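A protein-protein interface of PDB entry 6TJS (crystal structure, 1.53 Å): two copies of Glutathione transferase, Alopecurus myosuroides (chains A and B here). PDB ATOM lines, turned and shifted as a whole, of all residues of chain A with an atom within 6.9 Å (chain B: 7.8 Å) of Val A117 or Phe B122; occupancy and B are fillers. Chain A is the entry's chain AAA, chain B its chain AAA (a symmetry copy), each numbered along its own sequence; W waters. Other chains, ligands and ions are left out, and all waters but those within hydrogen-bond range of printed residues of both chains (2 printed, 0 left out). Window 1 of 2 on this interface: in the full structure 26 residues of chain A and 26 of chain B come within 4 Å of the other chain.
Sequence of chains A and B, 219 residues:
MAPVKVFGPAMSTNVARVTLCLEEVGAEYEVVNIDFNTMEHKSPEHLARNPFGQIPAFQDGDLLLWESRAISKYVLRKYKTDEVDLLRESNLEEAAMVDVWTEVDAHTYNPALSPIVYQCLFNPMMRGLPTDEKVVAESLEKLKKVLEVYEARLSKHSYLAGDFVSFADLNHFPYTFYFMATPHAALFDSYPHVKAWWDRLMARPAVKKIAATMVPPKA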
ATOM      1  N   MET A  11     -20.451 -17.749 -29.241  1.00  0.00           N
ATOM      2  CA  MET A  11     -21.617 -18.323 -28.527  1.00  0.00           C
ATOM      3  C   MET A  11     -21.580 -17.914 -27.039  1.00  0.00           C
ATOM      4  O   MET A  11     -22.567 -18.210 -26.333  1.00  0.00           O
ATOM      5  CB  MET A  11     -21.629 -19.851 -28.691  1.00  0.00           C
ATOM      6  CG  MET A  11     -20.649 -20.529 -27.785  1.00  0.00           C
ATOM      7  SD  MET A  11     -20.660 -22.331 -28.047  1.00  0.00           S
ATOM      8  CE  MET A  11     -22.083 -22.789 -27.055  1.00  0.00           C
ATOM      9  N   SER A  12     -20.494 -17.305 -26.506  1.00  0.00           N
ATOM     10  CA  SER A  12     -20.395 -16.849 -25.103  1.00  0.00           C
ATOM     11  C   SER A  12     -21.495 -15.820 -24.850  1.00  0.00           C
ATOM     12  O   SER A  12     -21.741 -14.938 -25.688  1.00  0.00           O
ATOM     13  CB  SER A  12     -19.026 -16.225 -24.837  1.00  0.00           C
ATOM     14  OG  SER A  12     -19.108 -15.177 -23.932  1.00  0.00           O
ATOM     15  N   THR A  13     -22.111 -15.907 -23.667  1.00  0.00           N
ATOM     16  CA  THR A  13     -23.167 -14.934 -23.313  1.00  0.00           C
ATOM     17  C   THR A  13     -22.581 -13.530 -23.302  1.00  0.00           C
ATOM     18  O   THR A  13     -23.310 -12.590 -23.710  1.00  0.00           O
ATOM     19  CB  THR A  13     -23.861 -15.307 -22.011  1.00  0.00           C
ATOM     20  OG1 THR A  13     -22.878 -15.386 -20.989  1.00  0.00           O
ATOM     21  CG2 THR A  13     -24.674 -16.577 -22.149  1.00  0.00           C
ATOM     22  N   ASN A  14     -21.385 -13.354 -22.788  1.00  0.00           N
ATOM     23  CA  ASN A  14     -20.781 -12.002 -22.699  1.00  0.00           C
ATOM     24  C   ASN A  14     -20.407 -11.462 -24.083  1.00  0.00           C
ATOM     25  O   ASN A  14     -20.491 -10.232 -24.332  1.00  0.00           O
ATOM     26  CB  ASN A  14     -19.611 -12.029 -21.747  1.00  0.00           C
ATOM     27  CG  ASN A  14     -20.090 -11.877 -20.320  1.00  0.00           C
ATOM     28  OD1 ASN A  14     -21.192 -11.412 -20.103  1.00  0.00           O
ATOM     29  ND2 ASN A  14     -19.308 -12.349 -19.365  1.00  0.00           N
ATOM     30  N   ALA A 112     -31.192 -16.826 -11.595  1.00  0.00           N
ATOM     31  CA  ALA A 112     -32.355 -17.736 -11.532  1.00  0.00           C
ATOM     32  C   ALA A 112     -32.305 -18.687 -12.731  1.00  0.00           C
ATOM     33  O   ALA A 112     -32.755 -19.827 -12.547  1.00  0.00           O
ATOM     34  CB  ALA A 112     -33.661 -16.997 -11.515  1.00  0.00           C
ATOM     35  N   LEU A 113     -31.805 -18.243 -13.896  1.00  0.00           N
ATOM     36  CA  LEU A 113     -31.778 -19.079 -15.130  1.00  0.00           C
ATOM     37  C   LEU A 113     -30.592 -20.010 -15.110  1.00  0.00           C
ATOM     38  O   LEU A 113     -30.756 -21.144 -15.605  1.00  0.00           O
ATOM     39  CB  LEU A 113     -31.627 -18.267 -16.428  1.00  0.00           C
ATOM     40  CG  LEU A 113     -32.888 -17.607 -16.916  1.00  0.00           C
ATOM     41  CD1 LEU A 113     -32.643 -16.946 -18.264  1.00  0.00           C
ATOM     42  CD2 LEU A 113     -34.062 -18.539 -16.966  1.00  0.00           C
ATOM     43  N   SER A 114     -29.435 -19.460 -14.738  1.00  0.00           N
ATOM     44  CA  SER A 114     -28.090 -19.930 -15.147  1.00  0.00           C
ATOM     45  C   SER A 114     -27.850 -21.381 -14.719  1.00  0.00           C
ATOM     46  O   SER A 114     -27.245 -22.132 -15.481  1.00  0.00           O
ATOM     47  CB  SER A 114     -27.005 -19.013 -14.650  1.00  0.00           C
ATOM     48  OG  SER A 114     -25.810 -19.257 -15.383  1.00  0.00           O
ATOM     49  N   PRO A 115     -28.297 -21.831 -13.525  1.00  0.00           N
ATOM     50  CA  PRO A 115     -27.971 -23.175 -13.062  1.00  0.00           C
ATOM     51  C   PRO A 115     -28.910 -24.193 -13.717  1.00  0.00           C
ATOM     52  O   PRO A 115     -28.511 -25.342 -13.892  1.00  0.00           O
ATOM     53  CB  PRO A 115     -28.135 -23.074 -11.539  1.00  0.00           C
ATOM     54  CG  PRO A 115     -29.235 -22.041 -11.350  1.00  0.00           C
ATOM     55  CD  PRO A 115     -29.095 -21.092 -12.527  1.00  0.00           C
ATOM     56  N   ILE A 116     -30.111 -23.762 -14.101  1.00  0.00           N
ATOM     57  CA  ILE A 116     -31.036 -24.577 -14.927  1.00  0.00           C
ATOM     58  C   ILE A 116     -30.394 -24.790 -16.298  1.00  0.00           C
ATOM     59  O   ILE A 116     -30.449 -25.921 -16.818  1.00  0.00           O
ATOM     60  CB  ILE A 116     -32.404 -23.906 -15.045  1.00  0.00           C
ATOM     61  CG1 ILE A 116     -33.058 -23.691 -13.677  1.00  0.00           C
ATOM     62  CG2 ILE A 116     -33.294 -24.668 -15.999  1.00  0.00           C
ATOM     63  CD1 ILE A 116     -34.020 -22.540 -13.649  1.00  0.00           C
ATOM     64  N   VAL A 117     -29.797 -23.755 -16.889  1.00  0.00           N
ATOM     65  CA  VAL A 117     -29.121 -23.936 -18.194  1.00  0.00           C
ATOM     66  C   VAL A 117     -27.956 -24.926 -18.000  1.00  0.00           C
ATOM     67  O   VAL A 117     -27.831 -25.841 -18.811  1.00  0.00           O
ATOM     68  CB  VAL A 117     -28.658 -22.588 -18.742  1.00  0.00           C
ATOM     69  CG1 VAL A 117     -27.677 -22.743 -19.877  1.00  0.00           C
ATOM     70  CG2 VAL A 117     -29.863 -21.709 -19.109  1.00  0.00           C
ATOM     71  N   TYR A 118     -27.110 -24.675 -17.008  1.00  0.00           N
ATOM     72  CA  TYR A 118     -25.890 -25.476 -16.731  1.00  0.00           C
ATOM     73  C   TYR A 118     -26.270 -26.944 -16.508  1.00  0.00           C
ATOM     74  O   TYR A 118     -25.694 -27.843 -17.195  1.00  0.00           O
ATOM     75  CB  TYR A 118     -25.210 -24.983 -15.456  1.00  0.00           C
ATOM     76  CG  TYR A 118     -24.348 -23.747 -15.569  1.00  0.00           C
ATOM     77  CD1 TYR A 118     -23.744 -23.349 -16.757  1.00  0.00           C
ATOM     78  CD2 TYR A 118     -24.084 -22.995 -14.429  1.00  0.00           C
ATOM     79  CE1 TYR A 118     -22.930 -22.227 -16.800  1.00  0.00           C
ATOM     80  CE2 TYR A 118     -23.273 -21.875 -14.459  1.00  0.00           C
ATOM     81  CZ  TYR A 118     -22.693 -21.493 -15.650  1.00  0.00           C
ATOM     82  OH  TYR A 118     -21.902 -20.384 -15.653  1.00  0.00           O
ATOM     83  N   GLN A 119     -27.182 -27.177 -15.585  1.00  0.00           N
ATOM     84  CA  GLN A 119     -27.697 -28.521 -15.211  1.00  0.00           C
ATOM     85  C   GLN A 119     -28.136 -29.233 -16.484  1.00  0.00           C
ATOM     86  O   GLN A 119     -27.634 -30.325 -16.767  1.00  0.00           O
ATOM     87  CB  GLN A 119     -28.837 -28.437 -14.188  1.00  0.00           C
ATOM     88  CG  GLN A 119     -29.832 -29.596 -14.231  1.00  0.00           C
ATOM     89  CD  GLN A 119     -29.265 -30.906 -13.739  1.00  0.00           C
ATOM     90  OE1 GLN A 119     -28.199 -30.956 -13.123  1.00  0.00           O
ATOM     91  NE2 GLN A 119     -29.989 -31.988 -13.997  1.00  0.00           N
ATOM     92  N   CSS A 120     -29.033 -28.580 -17.243  1.00  0.00           N
ATOM     93  CA  CSS A 120     -29.748 -29.213 -18.330  1.00  0.00           C
ATOM     94  CB  CSS A 120     -31.052 -28.496 -18.712  1.00  0.00           C
ATOM     95  SG  CSS A 120     -32.503 -28.748 -17.619  1.00  0.00           S
ATOM     96  SD  CSS A 120     -32.975 -30.740 -17.913  1.00  0.00           S
ATOM     97  C   CSS A 120     -28.793 -29.484 -19.501  1.00  0.00           C
ATOM     98  O   CSS A 120     -28.739 -30.601 -20.021  1.00  0.00           O
ATOM     99  N   LEU A 121     -27.956 -28.531 -19.883  1.00  0.00           N
ATOM    100  CA  LEU A 121     -27.203 -28.723 -21.101  1.00  0.00           C
ATOM    101  C   LEU A 121     -25.822 -29.335 -20.832  1.00  0.00           C
ATOM    102  O   LEU A 121     -25.259 -29.783 -21.863  1.00  0.00           O
ATOM    103  CB  LEU A 121     -27.097 -27.407 -21.876  1.00  0.00           C
ATOM    104  CG  LEU A 121     -28.439 -26.774 -22.254  1.00  0.00           C
ATOM    105  CD1 LEU A 121     -28.235 -25.430 -22.959  1.00  0.00           C
ATOM    106  CD2 LEU A 121     -29.284 -27.699 -23.120  1.00  0.00           C
ATOM    107  N   PHE A 122     -25.342 -29.358 -19.558  1.00  0.00           N
ATOM    108  CA  PHE A 122     -24.108 -30.072 -19.066  1.00  0.00           C
ATOM    109  C   PHE A 122     -24.184 -30.699 -17.662  1.00  0.00           C
ATOM    110  O   PHE A 122     -23.244 -30.408 -16.873  1.00  0.00           O
ATOM    111  CB  PHE A 122     -22.935 -29.113 -18.879  1.00  0.00           C
ATOM    112  CG  PHE A 122     -22.840 -28.080 -19.956  1.00  0.00           C
ATOM    113  CD1 PHE A 122     -23.684 -26.986 -19.957  1.00  0.00           C
ATOM    114  CD2 PHE A 122     -21.961 -28.236 -21.011  1.00  0.00           C
ATOM    115  CE1 PHE A 122     -23.660 -26.070 -20.985  1.00  0.00           C
ATOM    116  CE2 PHE A 122     -21.925 -27.297 -22.029  1.00  0.00           C
ATOM    117  CZ  PHE A 122     -22.760 -26.213 -22.008  1.00  0.00           C
ATOM    118  N   ASN A 123     -25.131 -31.596 -17.346  1.00  0.00           N
ATOM    119  CA  ASN A 123     -25.194 -32.302 -16.033  1.00  0.00           C
ATOM    120  C   ASN A 123     -24.078 -31.803 -15.091  1.00  0.00           C
ATOM    121  O   ASN A 123     -24.197 -30.628 -14.564  1.00  0.00           O
ATOM    122  CB  ASN A 123     -25.098 -33.791 -16.275  1.00  0.00           C
ATOM    123  N   PRO A 174     -29.074 -13.179 -24.142  1.00  0.00           N
ATOM    124  CA  PRO A 174     -28.165 -14.330 -24.243  1.00  0.00           C
ATOM    125  C   PRO A 174     -28.489 -15.507 -23.312  1.00  0.00           C
ATOM    126  O   PRO A 174     -28.571 -16.632 -23.799  1.00  0.00           O
ATOM    127  CB  PRO A 174     -26.801 -13.705 -23.894  1.00  0.00           C
ATOM    128  CG  PRO A 174     -26.934 -12.300 -24.382  1.00  0.00           C
ATOM    129  CD  PRO A 174     -28.343 -11.921 -23.932  1.00  0.00           C
ATOM    130  N   TYR A 175     -28.743 -15.259 -22.029  1.00  0.00           N
ATOM    131  CA  TYR A 175     -29.029 -16.357 -21.085  1.00  0.00           C
ATOM    132  C   TYR A 175     -30.400 -16.925 -21.395  1.00  0.00           C
ATOM    133  O   TYR A 175     -30.592 -18.149 -21.374  1.00  0.00           O
ATOM    134  CB  TYR A 175     -29.047 -15.899 -19.627  1.00  0.00           C
ATOM    135  CG  TYR A 175     -27.678 -15.881 -18.994  1.00  0.00           C
ATOM    136  CD1 TYR A 175     -26.818 -14.802 -19.181  1.00  0.00           C
ATOM    137  CD2 TYR A 175     -27.277 -16.888 -18.138  1.00  0.00           C
ATOM    138  CE1 TYR A 175     -25.557 -14.765 -18.600  1.00  0.00           C
ATOM    139  CE2 TYR A 175     -26.013 -16.874 -17.553  1.00  0.00           C
ATOM    140  CZ  TYR A 175     -25.156 -15.805 -17.770  1.00  0.00           C
ATOM    141  OH  TYR A 175     -23.911 -15.790 -17.184  1.00  0.00           O
ATOM    142  N   THR A 176     -31.374 -16.091 -21.720  1.00  0.00           N
ATOM    143  CA  THR A 176     -32.717 -16.626 -22.005  1.00  0.00           C
ATOM    144  C   THR A 176     -32.669 -17.500 -23.271  1.00  0.00           C
ATOM    145  O   THR A 176     -33.361 -18.518 -23.353  1.00  0.00           O
ATOM    146  CB  THR A 176     -33.757 -15.515 -22.186  1.00  0.00           C
ATOM    147  OG1 THR A 176     -33.626 -14.616 -21.079  1.00  0.00           O
ATOM    148  CG2 THR A 176     -35.165 -16.050 -22.262  1.00  0.00           C
ATOM    149  N   PHE A 177     -31.866 -17.142 -24.268  1.00  0.00           N
ATOM    150  CA  PHE A 177     -31.735 -17.948 -25.482  1.00  0.00           C
ATOM    151  C   PHE A 177     -31.314 -19.386 -25.096  1.00  0.00           C
ATOM    152  O   PHE A 177     -31.912 -20.330 -25.579  1.00  0.00           O
ATOM    153  CB  PHE A 177     -30.747 -17.261 -26.423  1.00  0.00           C
ATOM    154  CG  PHE A 177     -30.607 -17.963 -27.745  1.00  0.00           C
ATOM    155  CD1 PHE A 177     -31.656 -17.951 -28.637  1.00  0.00           C
ATOM    156  CD2 PHE A 177     -29.442 -18.625 -28.074  1.00  0.00           C
ATOM    157  CE1 PHE A 177     -31.566 -18.617 -29.851  1.00  0.00           C
ATOM    158  CE2 PHE A 177     -29.357 -19.287 -29.303  1.00  0.00           C
ATOM    159  CZ  PHE A 177     -30.400 -19.254 -30.174  1.00  0.00           C
ATOM    160  N   TYR A 178     -30.340 -19.527 -24.214  1.00  0.00           N
ATOM    161  CA  TYR A 178     -29.899 -20.860 -23.788  1.00  0.00           C
ATOM    162  C   TYR A 178     -30.961 -21.550 -22.936  1.00  0.00           C
ATOM    163  O   TYR A 178     -31.175 -22.747 -23.125  1.00  0.00           O
ATOM    164  CB  TYR A 178     -28.547 -20.803 -23.102  1.00  0.00           C
ATOM    165  CG  TYR A 178     -27.424 -20.593 -24.078  1.00  0.00           C
ATOM    166  CD1 TYR A 178     -27.245 -21.456 -25.129  1.00  0.00           C
ATOM    167  CD2 TYR A 178     -26.603 -19.499 -23.983  1.00  0.00           C
ATOM    168  CE1 TYR A 178     -26.257 -21.245 -26.077  1.00  0.00           C
ATOM    169  CE2 TYR A 178     -25.601 -19.266 -24.919  1.00  0.00           C
ATOM    170  CZ  TYR A 178     -25.396 -20.172 -25.945  1.00  0.00           C
ATOM    171  OH  TYR A 178     -24.428 -20.040 -26.898  1.00  0.00           O
ATOM    172  N   PHE A 179     -31.653 -20.802 -22.104  1.00  0.00           N
ATOM    173  CA  PHE A 179     -32.802 -21.382 -21.346  1.00  0.00           C
ATOM    174  C   PHE A 179     -33.824 -21.974 -22.278  1.00  0.00           C
ATOM    175  O   PHE A 179     -34.369 -23.081 -21.982  1.00  0.00           O
ATOM    176  CB  PHE A 179     -33.390 -20.338 -20.409  1.00  0.00           C
ATOM    177  CG  PHE A 179     -34.599 -20.866 -19.680  1.00  0.00           C
ATOM    178  CD1 PHE A 179     -34.439 -21.533 -18.499  1.00  0.00           C
ATOM    179  CD2 PHE A 179     -35.859 -20.698 -20.208  1.00  0.00           C
ATOM    180  CE1 PHE A 179     -35.557 -21.961 -17.785  1.00  0.00           C
ATOM    181  CE2 PHE A 179     -36.970 -21.157 -19.511  1.00  0.00           C
ATOM    182  CZ  PHE A 179     -36.806 -21.787 -18.321  1.00  0.00           C
ATOM    183  N   MET A 180     -34.076 -21.323 -23.408  1.00  0.00           N
ATOM    184  CA  MET A 180     -35.074 -21.762 -24.399  1.00  0.00           C
ATOM    185  C   MET A 180     -34.620 -23.033 -25.158  1.00  0.00           C
ATOM    186  O   MET A 180     -35.450 -23.689 -25.830  1.00  0.00           O
ATOM    187  CB  MET A 180     -35.419 -20.615 -25.347  1.00  0.00           C
ATOM    188  CG  MET A 180     -36.076 -19.493 -24.622  1.00  0.00           C
ATOM    189  SD  MET A 180     -37.700 -20.086 -23.974  1.00  0.00           S
ATOM    190  CE  MET A 180     -38.209 -18.686 -22.988  1.00  0.00           C
ATOM    191  N   THR A 182     -33.507 -25.605 -23.362  1.00  0.00           N
ATOM    192  CA  THR A 182     -33.728 -26.642 -22.323  1.00  0.00           C
ATOM    193  C   THR A 182     -35.167 -27.114 -22.375  1.00  0.00           C
ATOM    194  O   THR A 182     -36.030 -26.457 -22.926  1.00  0.00           O
ATOM    195  CB  THR A 182     -33.457 -26.126 -20.932  1.00  0.00           C
ATOM    196  OG1 THR A 182     -34.479 -25.255 -20.448  1.00  0.00           O
ATOM    197  CG2 THR A 182     -32.081 -25.516 -20.866  1.00  0.00           C
ATOM    198  N   MET B  11     -28.204 -30.356 -28.218  1.00  0.00           N
ATOM    199  CA  MET B  11     -26.881 -29.793 -27.858  1.00  0.00           C
ATOM    200  C   MET B  11     -26.490 -30.228 -26.430  1.00  0.00           C
ATOM    201  O   MET B  11     -25.342 -29.941 -26.031  1.00  0.00           O
ATOM    202  CB  MET B  11     -26.912 -28.262 -27.993  1.00  0.00           C
ATOM    203  CG  MET B  11     -27.590 -27.603 -26.832  1.00  0.00           C
ATOM    204  SD  MET B  11     -27.650 -25.796 -27.056  1.00  0.00           S
ATOM    205  CE  MET B  11     -26.001 -25.352 -26.504  1.00  0.00           C
ATOM    206  N   SER B  12     -27.380 -30.848 -25.618  1.00  0.00           N
ATOM    207  CA  SER B  12     -27.075 -31.329 -24.254  1.00  0.00           C
ATOM    208  C   SER B  12     -25.951 -32.359 -24.345  1.00  0.00           C
ATOM    209  O   SER B  12     -25.958 -33.226 -25.233  1.00  0.00           O
ATOM    210  CB  SER B  12     -28.311 -31.961 -23.619  1.00  0.00           C
ATOM    211  OG  SER B  12     -27.977 -33.025 -22.793  1.00  0.00           O
ATOM    212  N   SER B 114     -15.438 -28.875 -16.869  1.00  0.00           N
ATOM    213  CA  SER B 114     -16.842 -28.402 -16.867  1.00  0.00           C
ATOM    214  C   SER B 114     -16.946 -26.959 -16.363  1.00  0.00           C
ATOM    215  O   SER B 114     -17.742 -26.196 -16.907  1.00  0.00           O
ATOM    216  CB  SER B 114     -17.742 -29.331 -16.096  1.00  0.00           C
ATOM    217  OG  SER B 114     -19.097 -29.076 -16.452  1.00  0.00           O
ATOM    218  N   PRO B 115     -16.176 -26.529 -15.340  1.00  0.00           N
ATOM    219  CA  PRO B 115     -16.352 -25.194 -14.780  1.00  0.00           C
ATOM    220  C   PRO B 115     -15.636 -24.161 -15.658  1.00  0.00           C
ATOM    221  O   PRO B 115     -16.066 -23.011 -15.693  1.00  0.00           O
ATOM    222  CB  PRO B 115     -15.758 -25.321 -13.370  1.00  0.00           C
ATOM    223  CG  PRO B 115     -14.653 -26.354 -13.522  1.00  0.00           C
ATOM    224  CD  PRO B 115     -15.128 -27.282 -14.625  1.00  0.00           C
ATOM    225  N   ILE B 116     -14.597 -24.583 -16.378  1.00  0.00           N
ATOM    226  CA  ILE B 116     -13.946 -23.752 -17.420  1.00  0.00           C
ATOM    227  C   ILE B 116     -14.952 -23.517 -18.546  1.00  0.00           C
ATOM    228  O   ILE B 116     -15.045 -22.376 -19.040  1.00  0.00           O
ATOM    229  CB  ILE B 116     -12.670 -24.417 -17.936  1.00  0.00           C
ATOM    230  CG1 ILE B 116     -11.652 -24.654 -16.816  1.00  0.00           C
ATOM    231  CG2 ILE B 116     -12.089 -23.637 -19.091  1.00  0.00           C
ATOM    232  CD1 ILE B 116     -10.726 -25.803 -17.085  1.00  0.00           C
ATOM    233  N   VAL B 117     -15.697 -24.543 -18.959  1.00  0.00           N
ATOM    234  CA  VAL B 117     -16.717 -24.342 -20.012  1.00  0.00           C
ATOM    235  C   VAL B 117     -17.775 -23.358 -19.476  1.00  0.00           C
ATOM    236  O   VAL B 117     -18.125 -22.429 -20.201  1.00  0.00           O
ATOM    237  CB  VAL B 117     -17.321 -25.680 -20.428  1.00  0.00           C
ATOM    238  CG1 VAL B 117     -18.585 -25.509 -21.231  1.00  0.00           C
ATOM    239  CG2 VAL B 117     -16.274 -26.549 -21.140  1.00  0.00           C
ATOM    240  N   TYR B 118     -18.302 -23.628 -18.287  1.00  0.00           N
ATOM    241  CA  TYR B 118     -19.390 -22.835 -17.659  1.00  0.00           C
ATOM    242  C   TYR B 118     -18.959 -21.371 -17.528  1.00  0.00           C
ATOM    243  O   TYR B 118     -19.704 -20.460 -18.006  1.00  0.00           O
ATOM    244  CB  TYR B 118     -19.677 -23.352 -16.251  1.00  0.00           C
ATOM    245  CG  TYR B 118     -20.539 -24.588 -16.134  1.00  0.00           C
ATOM    246  CD1 TYR B 118     -21.459 -24.967 -17.106  1.00  0.00           C
ATOM    247  CD2 TYR B 118     -20.467 -25.359 -14.980  1.00  0.00           C
ATOM    248  CE1 TYR B 118     -22.253 -26.089 -16.933  1.00  0.00           C
ATOM    249  CE2 TYR B 118     -21.256 -26.481 -14.795  1.00  0.00           C
ATOM    250  CZ  TYR B 118     -22.153 -26.844 -15.776  1.00  0.00           C
ATOM    251  OH  TYR B 118     -22.915 -27.955 -15.573  1.00  0.00           O
ATOM    252  N   GLN B 119     -17.819 -21.150 -16.901  1.00  0.00           N
ATOM    253  CA  GLN B 119     -17.215 -19.812 -16.667  1.00  0.00           C
ATOM    254  C   GLN B 119     -17.158 -19.077 -18.000  1.00  0.00           C
ATOM    255  O   GLN B 119     -17.717 -17.981 -18.109  1.00  0.00           O
ATOM    256  CB  GLN B 119     -15.831 -19.911 -16.015  1.00  0.00           C
ATOM    257  CG  GLN B 119     -14.887 -18.749 -16.321  1.00  0.00           C
ATOM    258  CD  GLN B 119     -15.285 -17.449 -15.664  1.00  0.00           C
ATOM    259  OE1 GLN B 119     -16.130 -17.412 -14.768  1.00  0.00           O
ATOM    260  NE2 GLN B 119     -14.663 -16.361 -16.101  1.00  0.00           N
ATOM    261  N   CSS B 120     -16.517 -19.714 -18.995  1.00  0.00           N
ATOM    262  CA  CSS B 120     -16.142 -19.061 -20.231  1.00  0.00           C
ATOM    263  CB  CSS B 120     -15.003 -19.768 -20.982  1.00  0.00           C
ATOM    264  SG  CSS B 120     -13.300 -19.531 -20.346  1.00  0.00           S
ATOM    265  SD  CSS B 120     -12.927 -17.533 -20.728  1.00  0.00           S
ATOM    266  C   CSS B 120     -17.392 -18.772 -21.074  1.00  0.00           C
ATOM    267  O   CSS B 120     -17.589 -17.646 -21.537  1.00  0.00           O
ATOM    268  N   LEU B 121     -18.306 -19.720 -21.216  1.00  0.00           N
ATOM    269  CA  LEU B 121     -19.376 -19.509 -22.164  1.00  0.00           C
ATOM    270  C   LEU B 121     -20.620 -18.905 -21.501  1.00  0.00           C
ATOM    271  O   LEU B 121     -21.454 -18.441 -22.319  1.00  0.00           O
ATOM    272  CB  LEU B 121     -19.702 -20.811 -22.899  1.00  0.00           C
ATOM    273  CG  LEU B 121     -18.526 -21.435 -23.657  1.00  0.00           C
ATOM    274  CD1 LEU B 121     -18.927 -22.767 -24.298  1.00  0.00           C
ATOM    275  CD2 LEU B 121     -17.962 -20.493 -24.712  1.00  0.00           C
ATOM    276  N   PHE B 122     -20.714 -18.905 -20.142  1.00  0.00           N
ATOM    277  CA  PHE B 122     -21.754 -18.203 -19.305  1.00  0.00           C
ATOM    278  C   PHE B 122     -21.278 -17.601 -17.971  1.00  0.00           C
ATOM    279  O   PHE B 122     -21.953 -17.907 -16.951  1.00  0.00           O
ATOM    280  CB  PHE B 122     -22.828 -19.168 -18.807  1.00  0.00           C
ATOM    281  CG  PHE B 122     -23.230 -20.183 -19.829  1.00  0.00           C
ATOM    282  CD1 PHE B 122     -22.424 -21.275 -20.090  1.00  0.00           C
ATOM    283  CD2 PHE B 122     -24.373 -20.011 -20.585  1.00  0.00           C
ATOM    284  CE1 PHE B 122     -22.743 -22.172 -21.084  1.00  0.00           C
ATOM    285  CE2 PHE B 122     -24.702 -20.932 -21.566  1.00  0.00           C
ATOM    286  CZ  PHE B 122     -23.898 -22.014 -21.804  1.00  0.00           C
ATOM    287  N   ASN B 123     -20.277 -16.707 -17.924  1.00  0.00           N
ATOM    288  CA  ASN B 123     -19.840 -16.024 -16.672  1.00  0.00           C
ATOM    289  C   ASN B 123     -20.640 -16.542 -15.458  1.00  0.00           C
ATOM    290  O   ASN B 123     -20.379 -17.725 -15.008  1.00  0.00           O
ATOM    291  CB  ASN B 123     -19.997 -14.531 -16.850  1.00  0.00           C
ATOM    292  N   TYR B 178     -17.285 -28.642 -26.204  1.00  0.00           N
ATOM    293  CA  TYR B 178     -17.582 -27.317 -25.647  1.00  0.00           C
ATOM    294  C   TYR B 178     -16.318 -26.639 -25.123  1.00  0.00           C
ATOM    295  O   TYR B 178     -16.165 -25.439 -25.345  1.00  0.00           O
ATOM    296  CB  TYR B 178     -18.681 -27.390 -24.604  1.00  0.00           C
ATOM    297  CG  TYR B 178     -20.037 -27.586 -25.221  1.00  0.00           C
ATOM    298  CD1 TYR B 178     -20.507 -26.705 -26.162  1.00  0.00           C
ATOM    299  CD2 TYR B 178     -20.801 -28.683 -24.914  1.00  0.00           C
ATOM    300  CE1 TYR B 178     -21.726 -26.902 -26.790  1.00  0.00           C
ATOM    301  CE2 TYR B 178     -22.028 -28.902 -25.527  1.00  0.00           C
ATOM    302  CZ  TYR B 178     -22.515 -27.980 -26.435  1.00  0.00           C
ATOM    303  OH  TYR B 178     -23.718 -28.097 -27.074  1.00  0.00           O
HETATM  304  O   HOH W   1     -19.967 -15.469 -21.343  1.00  0.00           O
HETATM  305  O   HOH W   2     -26.411 -32.775 -20.553  1.00  0.00           O
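The backbone carbonyl oxygen of Leu B121 lies within hydrogen-bond range of the backbone NH of Thr A13 (2.9 Å). O of Tyr A118 is in hydrogen-bond range of OH of Tyr B118. The backbone carbonyl oxygen (O) of Phe B122 is in hydrogen-bond range of the side-chain hydroxyl (OH) of Tyr A118 (2.8 Å). The backbone carbonyl oxygen (O) of Asn B123 is in hydrogen-bond range of the side-chain hydroxyl (OH) of Tyr A118, 3.1 Å away. OH of Tyr B118 is in hydrogen-bond range of O of Phe A122 (2.8 Å). OH of Tyr B118 lies within hydrogen-bond range of O of Asn A123 (3.1 Å). The side-chain hydroxyl (OH) of Tyr A175 sits at hydrogen-bond distance from the backbone carbonyl oxygen (O) of Phe B122 (2.9 Å).
O of Met A11 lies within hydrogen-bond range of OH of Tyr A178 (2.7 Å). N of Asn A14 is in hydrogen-bond range of OG of Ser A12 (3.1 Å). The backbone carbonyl oxygen of Met B11 is in hydrogen-bond range of the side-chain hydroxyl of Tyr B178, at 2.7 Å.
Among the printed residues, merely in contact across the chains: Leu A121 with Ser B12 (3.4 Å), Ser A12 with Leu B121 (3.4 Å), Phe A122 with Tyr B178 (3.4 Å), Tyr A178 with Phe B122 (3.4 Å), Asn A14 with Asn B123 (3.4 Å), Thr A13 with Phe B122 (3.5 Å), Ser A12 with CSS B120 (3.8 Å), CSS A120 with Ser B12 (3.8 Å), Tyr A175 with Asn B123 (3.8 Å), Val A117 with Phe B122 (3.9 Å) and Phe A122 with Val B117 (3.9 Å).
Of the printed residues of chain B, Asn A14 touches Asn B123 (3.4 Å). Printed residues of chain B within 4 Å of Phe A122: Val B117 (3.9 Å), Tyr B118 (2.8 Å) and Tyr B178 (3.4 Å). Printed residues of chain A within 4 Å of Leu B121: Ser A12 (3.4 Å) and Thr A13 (2.9 Å). The nearest residue of chain B that does not touch Val A117 is Tyr B118 (5.9 Å). The nearest printed residue of chain A that does not touch Phe B122 is Phe A122 (4.01 Å).
Printed residues of chain A that touch a printed residue of chain B: Ser A12, Thr A13, Asn A14, Val A117, Tyr A118, CSS A120, Leu A121, Phe A122, Asn A123, Tyr A175 and Tyr A178. Hydrophobic or aromatic side chains of chain A that line the printed part of chain B: Val A117, Tyr A118, Phe A122, Tyr A175 and Tyr A178. Along chain B the printed residues that touch a printed residue of chain A span positions 12 to 178. Among the printed residues, 18 pairs touch across the chains.
Ser A12 touches CSS B120, and with the chains exchanged CSS A120 touches Ser B12. Tyr A118 touches Phe B122, and with the chains exchanged Phe A122 touches Tyr B118. Tyr A118 touches Asn B123, and with the chains exchanged Asn A123 touches Tyr B118.
Water W1 lies within hydrogen-bond range of the side-chain hydroxyl of Ser A12 (2.7 Å), the backbone NH of Asn A14 (2.9 Å), the side-chain hydroxyl of Thr A13 (2.9 Å), O of CSS B120 (3.2 Å) and the backbone carbonyl oxygen of Leu B121 (3.5 Å).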
